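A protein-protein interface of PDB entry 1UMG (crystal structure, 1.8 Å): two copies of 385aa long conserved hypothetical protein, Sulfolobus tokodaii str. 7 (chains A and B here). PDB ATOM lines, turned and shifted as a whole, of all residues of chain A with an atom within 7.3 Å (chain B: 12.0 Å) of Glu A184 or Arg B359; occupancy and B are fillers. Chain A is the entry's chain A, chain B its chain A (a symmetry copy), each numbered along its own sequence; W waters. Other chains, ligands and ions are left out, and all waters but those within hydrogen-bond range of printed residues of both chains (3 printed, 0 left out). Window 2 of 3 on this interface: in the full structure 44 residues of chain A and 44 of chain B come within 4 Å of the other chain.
The side-chain amino group (NZ) of Lys B355 lies within salt-bridge range of the side-chain carboxylate (OD2) of Asp A187 (3.2 Å). The backbone carbonyl oxygen of Met A178 lies within hydrogen-bond range of the guanidinium group of Arg B359, at 2.8 Å. O of Ala A176 sits at hydrogen-bond distance from N of Lys B361. The side-chain carboxylate of Glu A184 is in salt-bridge range of the guanidinium group of Arg B359 (2.6 Å).
N of Ser A180 is in hydrogen-bond range of OE1 of Glu A184 (2.9 Å).
Glu A175 touches Phe B360. CA of Glu A175 touches O of Lys B361 (3.1 Å). Lys B362 touches Glu A175. Ala A176 touches Arg B359. Ala A176 touches Phe B360 (O to CA, 3.5 Å). Val A177 touches Arg B359 (CG2 to CB, 3.9 Å). Phe B360 touches Val A177. Leu A179 touches Leu B356. CD1 of Ile B352 touches OD1 of Asp A187, 2.9 Å away. CD2 of Leu A189 touches CE2 of Phe B334, at 3.6 Å.
Glu A184 touches just one residue of chain B: Arg B359. Arg B359 touches five residues of chain A. Ala A176 touches three residues of chain B. Of chain B, only Arg B359 and Phe B360 come within 4 Å of Val A177. Met A178 touches one residue of chain B. Of chain B, only Leu B356 and Arg B359 come within 4 Å of Leu A179. No residue of chain B comes within 4 Å of Ser A180. Pro A182 touches none of the printed residues of chain B. Gln A183 touches none of the printed residues of chain B. No residue of chain B comes within 4 Å of Ile A185. Of chain B, only Ile B352 and Lys B355 come within 4 Å of Asp A187. No residue of chain B comes within 4 Å of Leu A188. Of the printed residues of chain A, Lys B355 touches Asp A187. Printed residues of chain A within 4 Å of Lys B361: Glu A175 (3.1 Å) and Ala A176 (2.8 Å). Of the printed residues of chain B, Glu A175 touches Phe B360, Lys B361 and Lys B362. Of the printed residues of chain A, Phe B360 touches Glu A175 (3.5 Å), Ala A176 (3.5 Å) and Val A177 (3.6 Å). Of the printed residues of chain A, Leu B356 touches Leu A179. Leu B351 touches none of the printed residues of chain A. The nearest residue of chain B that does not touch Glu A184 is Lys B355 (4.8 Å). The nearest printed residue of chain A that does not touch Leu B356 is Val A177 (4.3 Å).
Hydrophobic or aromatic side chains of chain A that line the printed part of chain B: Val A177, Leu A179 and Leu A189. Printed residues of chain B that touch a printed residue of chain A: Phe B334, Ile B352, Lys B355, Leu B356, Arg B359, Phe B360, Lys B361 and Lys B362. Among the printed residues, 15 pairs touch across the chains. Among the printed residues, Asp or Glu carboxylates within 4 Å of a Lys or Arg side-chain nitrogen of the other chain: Glu A184 with Arg B359 and Asp A187 with Lys B355.
No position is printed for both chains.
Water W3 bridges OD2 of Asp A187 and NZ of Lys B355. Water W2 bridges O of Pro B333 and O of Leu A189. Water W1 bridges O of Arg B359 (2.8 Å) and N of Met A178 (3.0 Å).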
ATOM      1  N   TYR A 142     -23.861 -17.975  18.870  1.00  0.00           N
ATOM      2  CA  TYR A 142     -23.244 -19.021  18.071  1.00  0.00           C
ATOM      3  C   TYR A 142     -23.160 -18.543  16.625  1.00  0.00           C
ATOM      4  O   TYR A 142     -22.136 -18.703  15.960  1.00  0.00           O
ATOM      5  CB  TYR A 142     -24.069 -20.310  18.110  1.00  0.00           C
ATOM      6  CG  TYR A 142     -23.562 -21.333  17.121  1.00  0.00           C
ATOM      7  CD1 TYR A 142     -22.414 -22.077  17.388  1.00  0.00           C
ATOM      8  CD2 TYR A 142     -24.177 -21.494  15.878  1.00  0.00           C
ATOM      9  CE1 TYR A 142     -21.886 -22.951  16.445  1.00  0.00           C
ATOM     10  CE2 TYR A 142     -23.655 -22.366  14.923  1.00  0.00           C
ATOM     11  CZ  TYR A 142     -22.510 -23.090  15.215  1.00  0.00           C
ATOM     12  OH  TYR A 142     -21.983 -23.944  14.277  1.00  0.00           O
ATOM     13  N   LYS A 165     -13.756 -18.588  20.618  1.00  0.00           N
ATOM     14  CA  LYS A 165     -14.020 -19.633  21.591  1.00  0.00           C
ATOM     15  C   LYS A 165     -15.107 -19.148  22.535  1.00  0.00           C
ATOM     16  O   LYS A 165     -15.229 -17.947  22.795  1.00  0.00           O
ATOM     17  CB  LYS A 165     -12.751 -20.013  22.358  1.00  0.00           C
ATOM     18  CG  LYS A 165     -12.028 -18.870  23.038  1.00  0.00           C
ATOM     19  CD  LYS A 165     -10.709 -19.379  23.601  1.00  0.00           C
ATOM     20  CE  LYS A 165      -9.858 -18.256  24.156  1.00  0.00           C
ATOM     21  NZ  LYS A 165      -8.529 -18.777  24.586  1.00  0.00           N
ATOM     22  N   GLU A 175     -20.089 -24.612  36.866  1.00  0.00           N
ATOM     23  CA  GLU A 175     -18.779 -24.808  36.253  1.00  0.00           C
ATOM     24  C   GLU A 175     -18.841 -24.373  34.796  1.00  0.00           C
ATOM     25  O   GLU A 175     -19.887 -24.479  34.156  1.00  0.00           O
ATOM     26  CB  GLU A 175     -18.370 -26.279  36.334  1.00  0.00           C
ATOM     27  CG  GLU A 175     -18.434 -26.857  37.739  1.00  0.00           C
ATOM     28  CD  GLU A 175     -17.926 -28.285  37.812  1.00  0.00           C
ATOM     29  OE1 GLU A 175     -18.028 -28.895  38.896  1.00  0.00           O
ATOM     30  OE2 GLU A 175     -17.421 -28.796  36.790  1.00  0.00           O
ATOM     31  N   ALA A 176     -17.719 -23.888  34.269  1.00  0.00           N
ATOM     32  CA  ALA A 176     -17.665 -23.430  32.887  1.00  0.00           C
ATOM     33  C   ALA A 176     -16.568 -24.114  32.085  1.00  0.00           C
ATOM     34  O   ALA A 176     -15.514 -24.471  32.614  1.00  0.00           O
ATOM     35  CB  ALA A 176     -17.469 -21.921  32.850  1.00  0.00           C
ATOM     36  N   VAL A 177     -16.827 -24.295  30.792  1.00  0.00           N
ATOM     37  CA  VAL A 177     -15.870 -24.923  29.897  1.00  0.00           C
ATOM     38  C   VAL A 177     -15.641 -24.015  28.690  1.00  0.00           C
ATOM     39  O   VAL A 177     -16.547 -23.289  28.271  1.00  0.00           O
ATOM     40  CB  VAL A 177     -16.381 -26.302  29.412  1.00  0.00           C
ATOM     41  CG1 VAL A 177     -17.667 -26.131  28.604  1.00  0.00           C
ATOM     42  CG2 VAL A 177     -15.310 -26.996  28.581  1.00  0.00           C
ATOM     43  N   MET A 178     -14.428 -24.044  28.152  1.00  0.00           N
ATOM     44  CA  MET A 178     -14.077 -23.237  26.985  1.00  0.00           C
ATOM     45  C   MET A 178     -14.040 -24.132  25.754  1.00  0.00           C
ATOM     46  O   MET A 178     -13.279 -25.097  25.704  1.00  0.00           O
ATOM     47  CB  MET A 178     -12.697 -22.590  27.166  1.00  0.00           C
ATOM     48  CG  MET A 178     -12.615 -21.519  28.237  1.00  0.00           C
ATOM     49  SD  MET A 178     -13.621 -20.065  27.869  1.00  0.00           S
ATOM     50  CE  MET A 178     -13.169 -19.756  26.194  1.00  0.00           C
ATOM     51  N   LEU A 179     -14.866 -23.812  24.761  1.00  0.00           N
ATOM     52  CA  LEU A 179     -14.905 -24.589  23.532  1.00  0.00           C
ATOM     53  C   LEU A 179     -14.553 -23.668  22.368  1.00  0.00           C
ATOM     54  O   LEU A 179     -15.069 -22.553  22.269  1.00  0.00           O
ATOM     55  CB  LEU A 179     -16.297 -25.205  23.340  1.00  0.00           C
ATOM     56  CG  LEU A 179     -16.691 -26.207  24.432  1.00  0.00           C
ATOM     57  CD1 LEU A 179     -18.149 -26.622  24.272  1.00  0.00           C
ATOM     58  CD2 LEU A 179     -15.776 -27.424  24.357  1.00  0.00           C
ATOM     59  N   SER A 180     -13.671 -24.137  21.494  1.00  0.00           N
ATOM     60  CA  SER A 180     -13.223 -23.344  20.361  1.00  0.00           C
ATOM     61  C   SER A 180     -13.828 -23.737  19.023  1.00  0.00           C
ATOM     62  O   SER A 180     -14.009 -24.917  18.724  1.00  0.00           O
ATOM     63  CB  SER A 180     -11.698 -23.413  20.238  1.00  0.00           C
ATOM     64  OG  SER A 180     -11.069 -22.949  21.421  1.00  0.00           O
ATOM     65  N   ALA A 181     -14.130 -22.723  18.218  1.00  0.00           N
ATOM     66  CA  ALA A 181     -14.670 -22.933  16.886  1.00  0.00           C
ATOM     67  C   ALA A 181     -13.580 -22.460  15.928  1.00  0.00           C
ATOM     68  O   ALA A 181     -12.849 -21.521  16.232  1.00  0.00           O
ATOM     69  CB  ALA A 181     -15.948 -22.113  16.698  1.00  0.00           C
ATOM     70  N   PRO A 182     -13.608 -23.066  15.055  1.00  0.00           N
ATOM     71  CA  PRO A 182     -14.522 -24.136  14.668  1.00  0.00           C
ATOM     72  C   PRO A 182     -14.625 -25.344  14.917  1.00  0.00           C
ATOM     73  O   PRO A 182     -15.223 -26.466  14.546  1.00  0.00           O
ATOM     74  CB  PRO A 182     -14.606 -23.959  13.171  1.00  0.00           C
ATOM     75  CG  PRO A 182     -13.149 -23.710  12.844  1.00  0.00           C
ATOM     76  CD  PRO A 182     -12.685 -22.755  13.949  1.00  0.00           C
ATOM     77  N   GLN A 183     -13.390 -26.038  15.581  1.00  0.00           N
ATOM     78  CA  GLN A 183     -13.201 -27.663  15.599  1.00  0.00           C
ATOM     79  C   GLN A 183     -14.017 -28.355  16.661  1.00  0.00           C
ATOM     80  O   GLN A 183     -14.148 -29.576  16.664  1.00  0.00           O
ATOM     81  CB  GLN A 183     -11.740 -27.482  16.053  1.00  0.00           C
ATOM     82  CG  GLN A 183     -11.531 -26.612  17.273  1.00  0.00           C
ATOM     83  CD  GLN A 183     -10.762 -25.338  16.950  1.00  0.00           C
ATOM     84  OE1 GLN A 183     -11.290 -24.425  16.319  1.00  0.00           O
ATOM     85  NE2 GLN A 183      -9.506 -25.281  17.378  1.00  0.00           N
ATOM     86  N   GLU A 184     -14.606 -27.558  17.545  1.00  0.00           N
ATOM     87  CA  GLU A 184     -15.424 -28.105  18.611  1.00  0.00           C
ATOM     88  C   GLU A 184     -16.870 -27.627  18.518  1.00  0.00           C
ATOM     89  O   GLU A 184     -17.592 -27.657  19.505  1.00  0.00           O
ATOM     90  CB  GLU A 184     -14.836 -27.726  19.972  1.00  0.00           C
ATOM     91  CG  GLU A 184     -13.387 -28.166  20.156  1.00  0.00           C
ATOM     92  CD  GLU A 184     -12.883 -27.965  21.574  1.00  0.00           C
ATOM     93  OE1 GLU A 184     -12.834 -26.808  22.041  1.00  0.00           O
ATOM     94  OE2 GLU A 184     -12.535 -28.975  22.223  1.00  0.00           O
ATOM     95  N   ILE A 185     -17.307 -27.205  17.336  1.00  0.00           N
ATOM     96  CA  ILE A 185     -18.680 -26.724  17.213  1.00  0.00           C
ATOM     97  C   ILE A 185     -19.747 -27.789  17.452  1.00  0.00           C
ATOM     98  O   ILE A 185     -20.821 -27.476  17.960  1.00  0.00           O
ATOM     99  CB  ILE A 185     -18.954 -26.055  15.840  1.00  0.00           C
ATOM    100  CG1 ILE A 185     -18.648 -27.028  14.706  1.00  0.00           C
ATOM    101  CG2 ILE A 185     -18.143 -24.769  15.714  1.00  0.00           C
ATOM    102  CD1 ILE A 185     -19.125 -26.535  13.348  1.00  0.00           C
ATOM    103  N   TYR A 186     -19.473 -29.043  17.095  1.00  0.00           N
ATOM    104  CA  TYR A 186     -20.473 -30.085  17.314  1.00  0.00           C
ATOM    105  C   TYR A 186     -20.607 -30.323  18.816  1.00  0.00           C
ATOM    106  O   TYR A 186     -21.706 -30.558  19.323  1.00  0.00           O
ATOM    107  CB  TYR A 186     -20.096 -31.385  16.582  1.00  0.00           C
ATOM    108  CG  TYR A 186     -19.960 -31.247  15.071  1.00  0.00           C
ATOM    109  CD1 TYR A 186     -20.619 -30.230  14.372  1.00  0.00           C
ATOM    110  CD2 TYR A 186     -19.170 -32.136  14.340  1.00  0.00           C
ATOM    111  CE1 TYR A 186     -20.486 -30.104  12.976  1.00  0.00           C
ATOM    112  CE2 TYR A 186     -19.031 -32.022  12.956  1.00  0.00           C
ATOM    113  CZ  TYR A 186     -19.688 -31.003  12.279  1.00  0.00           C
ATOM    114  OH  TYR A 186     -19.512 -30.879  10.916  1.00  0.00           O
ATOM    115  N   ASP A 187     -19.491 -30.240  19.533  1.00  0.00           N
ATOM    116  CA  ASP A 187     -19.507 -30.409  20.983  1.00  0.00           C
ATOM    117  C   ASP A 187     -20.243 -29.217  21.586  1.00  0.00           C
ATOM    118  O   ASP A 187     -21.103 -29.367  22.454  1.00  0.00           O
ATOM    119  CB  ASP A 187     -18.079 -30.438  21.531  1.00  0.00           C
ATOM    120  CG  ASP A 187     -17.239 -31.530  20.909  1.00  0.00           C
ATOM    121  OD1 ASP A 187     -17.574 -32.716  21.096  1.00  0.00           O
ATOM    122  OD2 ASP A 187     -16.247 -31.205  20.231  1.00  0.00           O
ATOM    123  N   LEU A 188     -19.887 -28.026  21.122  1.00  0.00           N
ATOM    124  CA  LEU A 188     -20.501 -26.800  21.605  1.00  0.00           C
ATOM    125  C   LEU A 188     -22.022 -26.850  21.469  1.00  0.00           C
ATOM    126  O   LEU A 188     -22.746 -26.601  22.431  1.00  0.00           O
ATOM    127  CB  LEU A 188     -19.957 -25.603  20.820  1.00  0.00           C
ATOM    128  CG  LEU A 188     -20.570 -24.234  21.120  1.00  0.00           C
ATOM    129  CD1 LEU A 188     -20.298 -23.834  22.562  1.00  0.00           C
ATOM    130  CD2 LEU A 188     -19.982 -23.208  20.161  1.00  0.00           C
ATOM    131  N   LEU A 189     -22.491 -27.174  20.270  1.00  0.00           N
ATOM    132  CA  LEU A 189     -23.922 -27.238  19.991  1.00  0.00           C
ATOM    133  C   LEU A 189     -24.655 -28.294  20.815  1.00  0.00           C
ATOM    134  O   LEU A 189     -25.813 -28.104  21.177  1.00  0.00           O
ATOM    135  CB  LEU A 189     -24.151 -27.474  18.491  1.00  0.00           C
ATOM    136  CG  LEU A 189     -23.768 -26.265  17.628  1.00  0.00           C
ATOM    137  CD1 LEU A 189     -23.774 -26.626  16.155  1.00  0.00           C
ATOM    138  CD2 LEU A 189     -24.742 -25.126  17.917  1.00  0.00           C
ATOM    139  N   ALA A 190     -23.979 -29.400  21.111  1.00  0.00           N
ATOM    140  CA  ALA A 190     -24.590 -30.460  21.906  1.00  0.00           C
ATOM    141  C   ALA A 190     -24.966 -29.894  23.269  1.00  0.00           C
ATOM    142  O   ALA A 190     -25.912 -30.358  23.907  1.00  0.00           O
ATOM    143  CB  ALA A 190     -23.619 -31.634  22.068  1.00  0.00           C
ATOM    144  N   PRO B 333     -29.950 -27.430  15.764  1.00  0.00           N
ATOM    145  CA  PRO B 333     -29.954 -28.305  16.944  1.00  0.00           C
ATOM    146  C   PRO B 333     -30.304 -27.630  18.269  1.00  0.00           C
ATOM    147  O   PRO B 333     -29.881 -28.085  19.330  1.00  0.00           O
ATOM    148  CB  PRO B 333     -28.534 -28.865  16.943  1.00  0.00           C
ATOM    149  CG  PRO B 333     -27.737 -27.665  16.519  1.00  0.00           C
ATOM    150  CD  PRO B 333     -28.572 -27.088  15.368  1.00  0.00           C
ATOM    151  N   PHE B 334     -31.077 -26.549  18.212  1.00  0.00           N
ATOM    152  CA  PHE B 334     -31.480 -25.826  19.419  1.00  0.00           C
ATOM    153  C   PHE B 334     -32.916 -26.107  19.840  1.00  0.00           C
ATOM    154  O   PHE B 334     -33.791 -26.285  18.994  1.00  0.00           O
ATOM    155  CB  PHE B 334     -31.352 -24.314  19.196  1.00  0.00           C
ATOM    156  CG  PHE B 334     -29.938 -23.812  19.199  1.00  0.00           C
ATOM    157  CD1 PHE B 334     -29.383 -23.285  20.361  1.00  0.00           C
ATOM    158  CD2 PHE B 334     -29.162 -23.868  18.046  1.00  0.00           C
ATOM    159  CE1 PHE B 334     -28.071 -22.813  20.374  1.00  0.00           C
ATOM    160  CE2 PHE B 334     -27.850 -23.403  18.045  1.00  0.00           C
ATOM    161  CZ  PHE B 334     -27.303 -22.875  19.216  1.00  0.00           C
ATOM    162  N   THR B 348     -25.425 -37.362  22.081  1.00  0.00           N
ATOM    163  CA  THR B 348     -23.986 -37.527  22.227  1.00  0.00           C
ATOM    164  C   THR B 348     -23.544 -36.828  23.515  1.00  0.00           C
ATOM    165  O   THR B 348     -22.364 -36.830  23.870  1.00  0.00           O
ATOM    166  CB  THR B 348     -23.239 -36.905  21.019  1.00  0.00           C
ATOM    167  OG1 THR B 348     -23.763 -37.452  19.801  1.00  0.00           O
ATOM    168  CG2 THR B 348     -21.749 -37.214  21.085  1.00  0.00           C
ATOM    169  N   LEU B 349     -24.512 -36.241  24.218  1.00  0.00           N
ATOM    170  CA  LEU B 349     -24.239 -35.514  25.453  1.00  0.00           C
ATOM    171  C   LEU B 349     -23.412 -36.295  26.473  1.00  0.00           C
ATOM    172  O   LEU B 349     -22.422 -35.779  26.993  1.00  0.00           O
ATOM    173  CB  LEU B 349     -25.550 -35.056  26.102  1.00  0.00           C
ATOM    174  CG  LEU B 349     -25.382 -34.203  27.362  1.00  0.00           C
ATOM    175  CD1 LEU B 349     -24.572 -32.959  27.029  1.00  0.00           C
ATOM    176  CD2 LEU B 349     -26.745 -33.818  27.918  1.00  0.00           C
ATOM    177  N   LEU B 351     -21.299 -38.664  26.102  1.00  0.00           N
ATOM    178  CA  LEU B 351     -19.935 -38.773  25.609  1.00  0.00           C
ATOM    179  C   LEU B 351     -19.197 -37.438  25.644  1.00  0.00           C
ATOM    180  O   LEU B 351     -18.000 -37.389  25.934  1.00  0.00           O
ATOM    181  CB  LEU B 351     -19.947 -39.328  24.182  1.00  0.00           C
ATOM    182  CG  LEU B 351     -20.569 -40.722  24.042  1.00  0.00           C
ATOM    183  CD1 LEU B 351     -20.634 -41.117  22.576  1.00  0.00           C
ATOM    184  CD2 LEU B 351     -19.742 -41.731  24.836  1.00  0.00           C
ATOM    185  N   ILE B 352     -19.913 -36.353  25.353  1.00  0.00           N
ATOM    186  CA  ILE B 352     -19.304 -35.028  25.359  1.00  0.00           C
ATOM    187  C   ILE B 352     -18.873 -34.641  26.771  1.00  0.00           C
ATOM    188  O   ILE B 352     -17.740 -34.211  26.983  1.00  0.00           O
ATOM    189  CB  ILE B 352     -20.278 -33.945  24.836  1.00  0.00           C
ATOM    190  CG1 ILE B 352     -20.723 -34.280  23.410  1.00  0.00           C
ATOM    191  CG2 ILE B 352     -19.604 -32.580  24.872  1.00  0.00           C
ATOM    192  CD1 ILE B 352     -19.586 -34.417  22.423  1.00  0.00           C
ATOM    193  N   LEU B 353     -19.779 -34.794  27.731  1.00  0.00           N
ATOM    194  CA  LEU B 353     -19.471 -34.453  29.114  1.00  0.00           C
ATOM    195  C   LEU B 353     -18.300 -35.287  29.629  1.00  0.00           C
ATOM    196  O   LEU B 353     -17.464 -34.798  30.391  1.00  0.00           O
ATOM    197  CB  LEU B 353     -20.701 -34.663  30.001  1.00  0.00           C
ATOM    198  CG  LEU B 353     -21.902 -33.767  29.673  1.00  0.00           C
ATOM    199  CD1 LEU B 353     -23.011 -34.009  30.681  1.00  0.00           C
ATOM    200  CD2 LEU B 353     -21.479 -32.305  29.695  1.00  0.00           C
ATOM    201  N   GLU B 354     -18.245 -36.545  29.206  1.00  0.00           N
ATOM    202  CA  GLU B 354     -17.157 -37.431  29.608  1.00  0.00           C
ATOM    203  C   GLU B 354     -15.850 -36.869  29.064  1.00  0.00           C
ATOM    204  O   GLU B 354     -14.844 -36.815  29.772  1.00  0.00           O
ATOM    205  CB  GLU B 354     -17.399 -38.841  29.059  1.00  0.00           C
ATOM    206  CG  GLU B 354     -16.258 -39.832  29.278  1.00  0.00           C
ATOM    207  CD  GLU B 354     -15.844 -39.953  30.733  1.00  0.00           C
ATOM    208  OE1 GLU B 354     -16.730 -39.939  31.613  1.00  0.00           O
ATOM    209  OE2 GLU B 354     -14.627 -40.075  30.996  1.00  0.00           O
ATOM    210  N   LYS B 355     -15.874 -36.440  27.806  1.00  0.00           N
ATOM    211  CA  LYS B 355     -14.689 -35.881  27.161  1.00  0.00           C
ATOM    212  C   LYS B 355     -14.245 -34.549  27.767  1.00  0.00           C
ATOM    213  O   LYS B 355     -13.058 -34.226  27.757  1.00  0.00           O
ATOM    214  CB  LYS B 355     -14.936 -35.672  25.663  1.00  0.00           C
ATOM    215  CG  LYS B 355     -13.731 -35.080  24.944  1.00  0.00           C
ATOM    216  CD  LYS B 355     -14.106 -33.961  23.978  1.00  0.00           C
ATOM    217  CE  LYS B 355     -14.218 -34.457  22.548  1.00  0.00           C
ATOM    218  NZ  LYS B 355     -14.348 -33.326  21.586  1.00  0.00           N
ATOM    219  N   LEU B 356     -15.196 -33.780  28.291  1.00  0.00           N
ATOM    220  CA  LEU B 356     -14.887 -32.471  28.867  1.00  0.00           C
ATOM    221  C   LEU B 356     -14.886 -32.440  30.396  1.00  0.00           C
ATOM    222  O   LEU B 356     -14.834 -31.365  30.993  1.00  0.00           O
ATOM    223  CB  LEU B 356     -15.894 -31.433  28.357  1.00  0.00           C
ATOM    224  CG  LEU B 356     -16.089 -31.291  26.844  1.00  0.00           C
ATOM    225  CD1 LEU B 356     -17.242 -30.334  26.572  1.00  0.00           C
ATOM    226  CD2 LEU B 356     -14.813 -30.790  26.193  1.00  0.00           C
ATOM    227  N   LYS B 357     -14.931 -33.608  31.030  1.00  0.00           N
ATOM    228  CA  LYS B 357     -14.966 -33.669  32.489  1.00  0.00           C
ATOM    229  C   LYS B 357     -13.852 -32.895  33.192  1.00  0.00           C
ATOM    230  O   LYS B 357     -14.083 -32.282  34.234  1.00  0.00           O
ATOM    231  CB  LYS B 357     -14.963 -35.126  32.961  1.00  0.00           C
ATOM    232  CG  LYS B 357     -13.720 -35.918  32.603  1.00  0.00           C
ATOM    233  CD  LYS B 357     -13.828 -37.333  33.148  1.00  0.00           C
ATOM    234  CE  LYS B 357     -12.584 -38.151  32.849  1.00  0.00           C
ATOM    235  NZ  LYS B 357     -12.694 -39.521  33.424  1.00  0.00           N
ATOM    236  N   ASP B 358     -12.647 -32.916  32.627  1.00  0.00           N
ATOM    237  CA  ASP B 358     -11.525 -32.208  33.236  1.00  0.00           C
ATOM    238  C   ASP B 358     -11.364 -30.776  32.733  1.00  0.00           C
ATOM    239  O   ASP B 358     -10.584 -30.002  33.289  1.00  0.00           O
ATOM    240  CB  ASP B 358     -10.222 -32.978  33.005  1.00  0.00           C
ATOM    241  CG  ASP B 358     -10.227 -34.339  33.670  1.00  0.00           C
ATOM    242  OD1 ASP B 358     -10.547 -34.410  34.875  1.00  0.00           O
ATOM    243  OD2 ASP B 358      -9.905 -35.337  32.990  1.00  0.00           O
ATOM    244  N   ARG B 359     -12.103 -30.421  31.685  1.00  0.00           N
ATOM    245  CA  ARG B 359     -12.021 -29.076  31.129  1.00  0.00           C
ATOM    246  C   ARG B 359     -13.015 -28.121  31.783  1.00  0.00           C
ATOM    247  O   ARG B 359     -12.895 -26.903  31.653  1.00  0.00           O
ATOM    248  CB  ARG B 359     -12.229 -29.123  29.614  1.00  0.00           C
ATOM    249  CG  ARG B 359     -11.106 -29.852  28.888  1.00  0.00           C
ATOM    250  CD  ARG B 359     -11.385 -30.003  27.407  1.00  0.00           C
ATOM    251  NE  ARG B 359     -11.572 -28.717  26.743  1.00  0.00           N
ATOM    252  CZ  ARG B 359     -11.776 -28.579  25.439  1.00  0.00           C
ATOM    253  NH1 ARG B 359     -11.813 -29.650  24.658  1.00  0.00           N
ATOM    254  NH2 ARG B 359     -11.943 -27.373  24.912  1.00  0.00           N
ATOM    255  N   PHE B 360     -13.998 -28.677  32.486  1.00  0.00           N
ATOM    256  CA  PHE B 360     -14.987 -27.867  33.189  1.00  0.00           C
ATOM    257  C   PHE B 360     -14.326 -27.341  34.460  1.00  0.00           C
ATOM    258  O   PHE B 360     -13.802 -28.117  35.259  1.00  0.00           O
ATOM    259  CB  PHE B 360     -16.211 -28.711  33.548  1.00  0.00           C
ATOM    260  CG  PHE B 360     -17.349 -28.578  32.573  1.00  0.00           C
ATOM    261  CD1 PHE B 360     -18.135 -27.431  32.558  1.00  0.00           C
ATOM    262  CD2 PHE B 360     -17.634 -29.600  31.672  1.00  0.00           C
ATOM    263  CE1 PHE B 360     -19.194 -27.303  31.663  1.00  0.00           C
ATOM    264  CE2 PHE B 360     -18.691 -29.481  30.771  1.00  0.00           C
ATOM    265  CZ  PHE B 360     -19.473 -28.330  30.767  1.00  0.00           C
ATOM    266  N   LYS B 361     -14.351 -26.023  34.644  1.00  0.00           N
ATOM    267  CA  LYS B 361     -13.725 -25.404  35.808  1.00  0.00           C
ATOM    268  C   LYS B 361     -14.728 -24.833  36.808  1.00  0.00           C
ATOM    269  O   LYS B 361     -15.750 -24.265  36.424  1.00  0.00           O
ATOM    270  CB  LYS B 361     -12.775 -24.295  35.349  1.00  0.00           C
ATOM    271  CG  LYS B 361     -11.788 -24.728  34.271  1.00  0.00           C
ATOM    272  CD  LYS B 361     -10.864 -25.830  34.769  1.00  0.00           C
ATOM    273  CE  LYS B 361      -9.966 -26.358  33.657  1.00  0.00           C
ATOM    274  NZ  LYS B 361      -9.076 -25.308  33.089  1.00  0.00           N
ATOM    275  N   LYS B 362     -14.421 -24.988  38.091  1.00  0.00           N
ATOM    276  CA  LYS B 362     -15.279 -24.485  39.161  1.00  0.00           C
ATOM    277  C   LYS B 362     -15.045 -22.990  39.356  1.00  0.00           C
ATOM    278  O   LYS B 362     -16.013 -22.218  39.197  1.00  0.00           O
ATOM    279  CB  LYS B 362     -14.978 -25.222  40.470  1.00  0.00           C
ATOM    280  CG  LYS B 362     -15.397 -26.687  40.487  1.00  0.00           C
ATOM    281  CD  LYS B 362     -16.897 -26.841  40.693  1.00  0.00           C
ATOM    282  CE  LYS B 362     -17.330 -26.333  42.062  1.00  0.00           C
ATOM    283  NZ  LYS B 362     -18.792 -26.511  42.291  1.00  0.00           N
ATOM    284  OXT LYS B 362     -13.896 -22.611  39.666  1.00  0.00           O
HETATM  285  O   HOH W   1     -12.099 -25.095  29.733  1.00  0.00           O
HETATM  286  O   HOH W   2     -28.119 -29.678  20.711  1.00  0.00           O
HETATM  287  O   HOH W   3     -14.904 -32.600  18.463  1.00  0.00           O
